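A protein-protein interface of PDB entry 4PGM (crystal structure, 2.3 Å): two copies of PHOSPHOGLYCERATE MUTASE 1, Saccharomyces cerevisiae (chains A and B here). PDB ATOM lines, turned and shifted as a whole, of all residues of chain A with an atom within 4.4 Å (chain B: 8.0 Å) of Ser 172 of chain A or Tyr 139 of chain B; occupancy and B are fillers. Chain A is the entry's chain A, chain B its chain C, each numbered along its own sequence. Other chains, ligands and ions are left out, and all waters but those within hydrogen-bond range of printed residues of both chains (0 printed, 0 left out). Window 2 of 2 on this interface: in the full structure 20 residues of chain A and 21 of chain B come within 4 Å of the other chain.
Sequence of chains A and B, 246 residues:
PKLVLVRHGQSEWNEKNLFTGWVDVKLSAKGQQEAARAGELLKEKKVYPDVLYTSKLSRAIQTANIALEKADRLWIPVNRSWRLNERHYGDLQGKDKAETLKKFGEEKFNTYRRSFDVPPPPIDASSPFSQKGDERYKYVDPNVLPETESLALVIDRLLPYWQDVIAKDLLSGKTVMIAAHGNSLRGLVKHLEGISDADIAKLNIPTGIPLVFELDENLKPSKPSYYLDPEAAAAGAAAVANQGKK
Of the 8 printed residues of chain A, 4 touch a printed residue of chain B. Hydrophobic or aromatic side chains of chain A within 4 Å of the printed part of chain B: Ala 167 and Leu 171. Along chain A the printed residues that touch a printed residue of chain B span positions 167 to 172. Of the 12 printed residues of chain B, 4 touch a printed residue of chain A. Hydrophobic or aromatic side chains of chain B within 4 Å of the printed part of chain A: Tyr 139. Among the printed residues, 7 pairs touch across the chains. Among the printed residues, no Asp or Glu carboxylate lies within 4 Å of a Lys or Arg side-chain nitrogen of the other chain.
No position is printed for both chains. Of the 7 pairs that touch across the chains among the printed residues, none has its exchanged pair printed and touching as well.
The backbone NH of Lys 168 of chain A lies close to the backbone carbonyl oxygen of Tyr 139 of chain B (3.5 Å).
Printed residues of chain B within 4 Å of Lys 168 of chain A: Tyr 139. Of the printed residues of chain B, Leu 171 of chain A touches Lys 138, Tyr 139 and Val 140. Of chain B, only Tyr 139 comes within 4 Å of Ser 172 of chain A. Lys 56 of chain B touches none of the printed residues of chain A. Of the printed residues of chain A, Lys 138 of chain B touches Leu 171 (3.4 Å). Tyr 139 of chain B touches just these residues of chain A: Ala 167 (3.8 Å), Lys 168 (3.4 Å), Leu 171 (3.4 Å) and Ser 172 (3.3 Å). Of the printed residues of chain A, Val 140 of chain B touches Leu 171. Of the printed residues of chain A, Asp 141 of chain B touches Ala 167. The nearest printed residue of chain A that does not touch Tyr 139 of chain B is Asp 169 of chain A (5.8 Å). The nearest printed residue of chain A that does not touch Asp 141 of chain B is Leu 171 of chain A (4.4 Å).
O of Tyr 139 of chain B touches C of Ala 167 of chain A, 3.8 Å away. Asp 141 of chain B touches Ala 167 of chain A (N to CB, 3.8 Å). Leu 171 of chain A touches Lys 138 of chain B (CD1 to O, 3.4 Å). Tyr 139 of chain B touches Leu 171 of chain A (C to CD1, 3.4 Å). Val 140 of chain B touches Leu 171 of chain A (O to CD1, 3.5 Å). Tyr 139 of chain B touches Ser 172 of chain A (CE1 to OG, 3.3 Å).
O of Lys 168 of chain A sits at hydrogen-bond distance from OG of Ser 172 of chain A.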
ATOM      1  N   ALA A 167       5.663  -2.251 -30.955  1.00  0.00           N
ATOM      2  CA  ALA A 167       6.107  -0.868 -31.134  1.00  0.00           C
ATOM      3  C   ALA A 167       6.214  -0.094 -29.809  1.00  0.00           C
ATOM      4  O   ALA A 167       7.142   0.683 -29.631  1.00  0.00           O
ATOM      5  CB  ALA A 167       5.165  -0.135 -32.048  1.00  0.00           C
ATOM      6  N   LYS A 168       5.291  -0.332 -28.872  1.00  0.00           N
ATOM      7  CA  LYS A 168       5.295   0.357 -27.577  1.00  0.00           C
ATOM      8  C   LYS A 168       6.507   0.031 -26.733  1.00  0.00           C
ATOM      9  O   LYS A 168       7.141   0.937 -26.166  1.00  0.00           O
ATOM     10  CB  LYS A 168       4.022   0.045 -26.793  1.00  0.00           C
ATOM     11  CG  LYS A 168       3.892   0.808 -25.470  1.00  0.00           C
ATOM     12  CD  LYS A 168       2.456   0.762 -24.949  1.00  0.00           C
ATOM     13  CE  LYS A 168       2.238   1.853 -23.898  1.00  0.00           C
ATOM     14  NZ  LYS A 168       0.804   2.312 -23.810  1.00  0.00           N
ATOM     15  N   ASP A 169       6.832  -1.257 -26.629  1.00  0.00           N
ATOM     16  CA  ASP A 169       8.013  -1.658 -25.849  1.00  0.00           C
ATOM     17  C   ASP A 169       9.287  -1.172 -26.530  1.00  0.00           C
ATOM     18  O   ASP A 169      10.208  -0.686 -25.879  1.00  0.00           O
ATOM     19  CB  ASP A 169       8.073  -3.170 -25.652  1.00  0.00           C
ATOM     20  CG  ASP A 169       7.055  -3.667 -24.642  1.00  0.00           C
ATOM     21  OD1 ASP A 169       6.777  -2.976 -23.632  1.00  0.00           O
ATOM     22  OD2 ASP A 169       6.523  -4.764 -24.857  1.00  0.00           O
ATOM     23  N   LEU A 170       9.285  -1.223 -27.856  1.00  0.00           N
ATOM     24  CA  LEU A 170      10.423  -0.776 -28.641  1.00  0.00           C
ATOM     25  C   LEU A 170      10.639   0.717 -28.389  1.00  0.00           C
ATOM     26  O   LEU A 170      11.742   1.139 -28.050  1.00  0.00           O
ATOM     27  CB  LEU A 170      10.161  -1.075 -30.121  1.00  0.00           C
ATOM     28  CG  LEU A 170      11.091  -1.960 -30.979  1.00  0.00           C
ATOM     29  CD1 LEU A 170      12.092  -2.774 -30.181  1.00  0.00           C
ATOM     30  CD2 LEU A 170      10.246  -2.870 -31.817  1.00  0.00           C
ATOM     31  N   LEU A 171       9.563   1.497 -28.484  1.00  0.00           N
ATOM     32  CA  LEU A 171       9.613   2.940 -28.253  1.00  0.00           C
ATOM     33  C   LEU A 171       9.815   3.299 -26.756  1.00  0.00           C
ATOM     34  O   LEU A 171       9.990   4.475 -26.414  1.00  0.00           O
ATOM     35  CB  LEU A 171       8.347   3.614 -28.820  1.00  0.00           C
ATOM     36  CG  LEU A 171       8.174   3.612 -30.353  1.00  0.00           C
ATOM     37  CD1 LEU A 171       6.745   3.896 -30.785  1.00  0.00           C
ATOM     38  CD2 LEU A 171       9.159   4.560 -30.991  1.00  0.00           C
ATOM     39  N   SER A 172       9.777   2.299 -25.869  1.00  0.00           N
ATOM     40  CA  SER A 172       9.999   2.506 -24.433  1.00  0.00           C
ATOM     41  C   SER A 172      11.420   2.078 -24.038  1.00  0.00           C
ATOM     42  O   SER A 172      11.733   1.982 -22.846  1.00  0.00           O
ATOM     43  CB  SER A 172       9.013   1.698 -23.585  1.00  0.00           C
ATOM     44  OG  SER A 172       7.664   2.086 -23.757  1.00  0.00           O
ATOM     45  N   GLY A 173      12.253   1.751 -25.020  1.00  0.00           N
ATOM     46  CA  GLY A 173      13.622   1.348 -24.725  1.00  0.00           C
ATOM     47  C   GLY A 173      13.788  -0.104 -24.300  1.00  0.00           C
ATOM     48  O   GLY A 173      14.851  -0.518 -23.823  1.00  0.00           O
ATOM     49  N   LYS A 174      12.740  -0.890 -24.481  1.00  0.00           N
ATOM     50  CA  LYS A 174      12.773  -2.290 -24.109  1.00  0.00           C
ATOM     51  C   LYS A 174      13.343  -3.070 -25.287  1.00  0.00           C
ATOM     52  O   LYS A 174      12.789  -2.983 -26.379  1.00  0.00           O
ATOM     53  CB  LYS A 174      11.356  -2.780 -23.876  1.00  0.00           C
ATOM     54  CG  LYS A 174      10.935  -2.903 -22.445  1.00  0.00           C
ATOM     55  CD  LYS A 174      10.648  -1.575 -21.810  1.00  0.00           C
ATOM     56  CE  LYS A 174       9.853  -1.798 -20.526  1.00  0.00           C
ATOM     57  NZ  LYS A 174       9.475  -0.527 -19.903  1.00  0.00           N
ATOM     58  N   LYS B  56      -8.883   8.023 -28.476  1.00  0.00           N
ATOM     59  CA  LYS B  56      -7.972   8.904 -27.749  1.00  0.00           C
ATOM     60  C   LYS B  56      -8.414  10.384 -27.855  1.00  0.00           C
ATOM     61  O   LYS B  56      -7.687  11.293 -27.464  1.00  0.00           O
ATOM     62  CB  LYS B  56      -6.552   8.734 -28.285  1.00  0.00           C
ATOM     63  CG  LYS B  56      -5.927   7.394 -27.900  1.00  0.00           C
ATOM     64  CD  LYS B  56      -4.565   7.611 -27.267  1.00  0.00           C
ATOM     65  CE  LYS B  56      -3.864   6.304 -26.961  1.00  0.00           C
ATOM     66  NZ  LYS B  56      -4.587   5.504 -25.946  1.00  0.00           N
ATOM     67  N   TRP B  82      -6.064   4.553 -30.454  1.00  0.00           N
ATOM     68  CA  TRP B  82      -6.043   5.437 -31.607  1.00  0.00           C
ATOM     69  C   TRP B  82      -6.907   4.766 -32.688  1.00  0.00           C
ATOM     70  O   TRP B  82      -7.465   5.451 -33.551  1.00  0.00           O
ATOM     71  CB  TRP B  82      -4.608   5.616 -32.123  1.00  0.00           C
ATOM     72  CG  TRP B  82      -4.046   4.409 -32.885  1.00  0.00           C
ATOM     73  CD1 TRP B  82      -3.325   3.370 -32.366  1.00  0.00           C
ATOM     74  CD2 TRP B  82      -4.161   4.143 -34.295  1.00  0.00           C
ATOM     75  NE1 TRP B  82      -2.976   2.481 -33.360  1.00  0.00           N
ATOM     76  CE2 TRP B  82      -3.484   2.926 -34.553  1.00  0.00           C
ATOM     77  CE3 TRP B  82      -4.774   4.812 -35.369  1.00  0.00           C
ATOM     78  CZ2 TRP B  82      -3.407   2.366 -35.839  1.00  0.00           C
ATOM     79  CZ3 TRP B  82      -4.694   4.253 -36.648  1.00  0.00           C
ATOM     80  CH2 TRP B  82      -4.018   3.043 -36.866  1.00  0.00           C
ATOM     81  N   ASP B 134       1.919  13.848 -31.938  1.00  0.00           N
ATOM     82  CA  ASP B 134       1.146  14.162 -30.756  1.00  0.00           C
ATOM     83  C   ASP B 134       1.480  13.209 -29.591  1.00  0.00           C
ATOM     84  O   ASP B 134       1.568  11.982 -29.764  1.00  0.00           O
ATOM     85  CB  ASP B 134      -0.344  14.074 -31.084  1.00  0.00           C
ATOM     86  CG  ASP B 134      -1.206  14.833 -30.108  1.00  0.00           C
ATOM     87  OD1 ASP B 134      -1.229  14.485 -28.906  1.00  0.00           O
ATOM     88  OD2 ASP B 134      -1.868  15.793 -30.546  1.00  0.00           O
ATOM     89  N   GLU B 135       1.541  13.777 -28.389  1.00  0.00           N
ATOM     90  CA  GLU B 135       1.875  13.035 -27.181  1.00  0.00           C
ATOM     91  C   GLU B 135       1.109  11.733 -26.979  1.00  0.00           C
ATOM     92  O   GLU B 135       1.704  10.717 -26.599  1.00  0.00           O
ATOM     93  CB  GLU B 135       1.700  13.908 -25.935  1.00  0.00           C
ATOM     94  CG  GLU B 135       2.463  13.375 -24.728  1.00  0.00           C
ATOM     95  CD  GLU B 135       2.105  14.052 -23.419  1.00  0.00           C
ATOM     96  OE1 GLU B 135       1.619  15.199 -23.440  1.00  0.00           O
ATOM     97  OE2 GLU B 135       2.305  13.423 -22.353  1.00  0.00           O
ATOM     98  N   ARG B 136      -0.197  11.751 -27.250  1.00  0.00           N
ATOM     99  CA  ARG B 136      -1.010  10.566 -27.053  1.00  0.00           C
ATOM    100  C   ARG B 136      -0.719   9.419 -28.045  1.00  0.00           C
ATOM    101  O   ARG B 136      -1.284   8.337 -27.910  1.00  0.00           O
ATOM    102  CB  ARG B 136      -2.497  10.929 -27.037  1.00  0.00           C
ATOM    103  CG  ARG B 136      -3.035  11.416 -28.379  1.00  0.00           C
ATOM    104  CD  ARG B 136      -4.373  12.104 -28.215  1.00  0.00           C
ATOM    105  NE  ARG B 136      -4.215  13.498 -27.815  1.00  0.00           N
ATOM    106  CZ  ARG B 136      -5.190  14.242 -27.307  1.00  0.00           C
ATOM    107  NH1 ARG B 136      -6.411  13.738 -27.117  1.00  0.00           N
ATOM    108  NH2 ARG B 136      -4.943  15.491 -26.989  1.00  0.00           N
ATOM    109  N   TYR B 137       0.142   9.648 -29.038  1.00  0.00           N
ATOM    110  CA  TYR B 137       0.494   8.608 -30.021  1.00  0.00           C
ATOM    111  C   TYR B 137       1.999   8.295 -30.053  1.00  0.00           C
ATOM    112  O   TYR B 137       2.466   7.621 -30.969  1.00  0.00           O
ATOM    113  CB  TYR B 137       0.052   9.011 -31.444  1.00  0.00           C
ATOM    114  CG  TYR B 137      -1.385   9.491 -31.550  1.00  0.00           C
ATOM    115  CD1 TYR B 137      -2.445   8.633 -31.282  1.00  0.00           C
ATOM    116  CD2 TYR B 137      -1.678  10.820 -31.863  1.00  0.00           C
ATOM    117  CE1 TYR B 137      -3.763   9.081 -31.316  1.00  0.00           C
ATOM    118  CE2 TYR B 137      -2.983  11.272 -31.902  1.00  0.00           C
ATOM    119  CZ  TYR B 137      -4.024  10.394 -31.623  1.00  0.00           C
ATOM    120  OH  TYR B 137      -5.335  10.812 -31.622  1.00  0.00           O
ATOM    121  N   LYS B 138       2.748   8.720 -29.039  1.00  0.00           N
ATOM    122  CA  LYS B 138       4.211   8.521 -29.019  1.00  0.00           C
ATOM    123  C   LYS B 138       4.662   7.067 -28.924  1.00  0.00           C
ATOM    124  O   LYS B 138       5.803   6.734 -29.250  1.00  0.00           O
ATOM    125  CB  LYS B 138       4.846   9.330 -27.883  1.00  0.00           C
ATOM    126  CG  LYS B 138       4.370   8.914 -26.496  1.00  0.00           C
ATOM    127  CD  LYS B 138       4.657   9.971 -25.447  1.00  0.00           C
ATOM    128  CE  LYS B 138       6.138  10.202 -25.262  1.00  0.00           C
ATOM    129  NZ  LYS B 138       6.401  10.886 -23.956  1.00  0.00           N
ATOM    130  N   TYR B 139       3.781   6.210 -28.431  1.00  0.00           N
ATOM    131  CA  TYR B 139       4.113   4.812 -28.295  1.00  0.00           C
ATOM    132  C   TYR B 139       3.582   3.970 -29.446  1.00  0.00           C
ATOM    133  O   TYR B 139       3.781   2.765 -29.464  1.00  0.00           O
ATOM    134  CB  TYR B 139       3.617   4.290 -26.948  1.00  0.00           C
ATOM    135  CG  TYR B 139       4.429   4.817 -25.786  1.00  0.00           C
ATOM    136  CD1 TYR B 139       5.790   4.539 -25.685  1.00  0.00           C
ATOM    137  CD2 TYR B 139       3.855   5.635 -24.824  1.00  0.00           C
ATOM    138  CE1 TYR B 139       6.569   5.072 -24.657  1.00  0.00           C
ATOM    139  CE2 TYR B 139       4.619   6.174 -23.790  1.00  0.00           C
ATOM    140  CZ  TYR B 139       5.978   5.894 -23.714  1.00  0.00           C
ATOM    141  OH  TYR B 139       6.746   6.473 -22.722  1.00  0.00           O
ATOM    142  N   VAL B 140       2.917   4.599 -30.411  1.00  0.00           N
ATOM    143  CA  VAL B 140       2.374   3.871 -31.559  1.00  0.00           C
ATOM    144  C   VAL B 140       3.365   3.944 -32.720  1.00  0.00           C
ATOM    145  O   VAL B 140       4.099   4.927 -32.835  1.00  0.00           O
ATOM    146  CB  VAL B 140       1.011   4.465 -31.989  1.00  0.00           C
ATOM    147  CG1 VAL B 140       0.444   3.735 -33.205  1.00  0.00           C
ATOM    148  CG2 VAL B 140       0.039   4.382 -30.824  1.00  0.00           C
ATOM    149  N   ASP B 141       3.448   2.889 -33.529  1.00  0.00           N
ATOM    150  CA  ASP B 141       4.368   2.912 -34.687  1.00  0.00           C
ATOM    151  C   ASP B 141       4.086   4.180 -35.504  1.00  0.00           C
ATOM    152  O   ASP B 141       3.008   4.301 -36.102  1.00  0.00           O
ATOM    153  CB  ASP B 141       4.147   1.660 -35.562  1.00  0.00           C
ATOM    154  CG  ASP B 141       5.034   1.623 -36.825  1.00  0.00           C
ATOM    155  OD1 ASP B 141       6.035   2.376 -36.950  1.00  0.00           O
ATOM    156  OD2 ASP B 141       4.704   0.811 -37.719  1.00  0.00           O
ATOM    157  N   PRO B 142       5.053   5.129 -35.556  1.00  0.00           N
ATOM    158  CA  PRO B 142       4.892   6.387 -36.300  1.00  0.00           C
ATOM    159  C   PRO B 142       4.269   6.207 -37.688  1.00  0.00           C
ATOM    160  O   PRO B 142       3.328   6.903 -38.059  1.00  0.00           O
ATOM    161  CB  PRO B 142       6.324   6.896 -36.416  1.00  0.00           C
ATOM    162  CG  PRO B 142       6.974   6.410 -35.146  1.00  0.00           C
ATOM    163  CD  PRO B 142       6.434   5.007 -35.033  1.00  0.00           C
ATOM    164  N   LEU B 145       0.186   5.651 -38.238  1.00  0.00           N
ATOM    165  CA  LEU B 145      -0.608   6.855 -37.995  1.00  0.00           C
ATOM    166  C   LEU B 145      -0.816   7.599 -39.316  1.00  0.00           C
ATOM    167  O   LEU B 145       0.146   7.981 -39.994  1.00  0.00           O
ATOM    168  CB  LEU B 145       0.096   7.734 -36.944  1.00  0.00           C
ATOM    169  CG  LEU B 145      -0.148   7.574 -35.403  1.00  0.00           C
ATOM    170  CD1 LEU B 145      -1.042   6.446 -35.022  1.00  0.00           C
ATOM    171  CD2 LEU B 145       1.132   7.473 -34.618  1.00  0.00           C
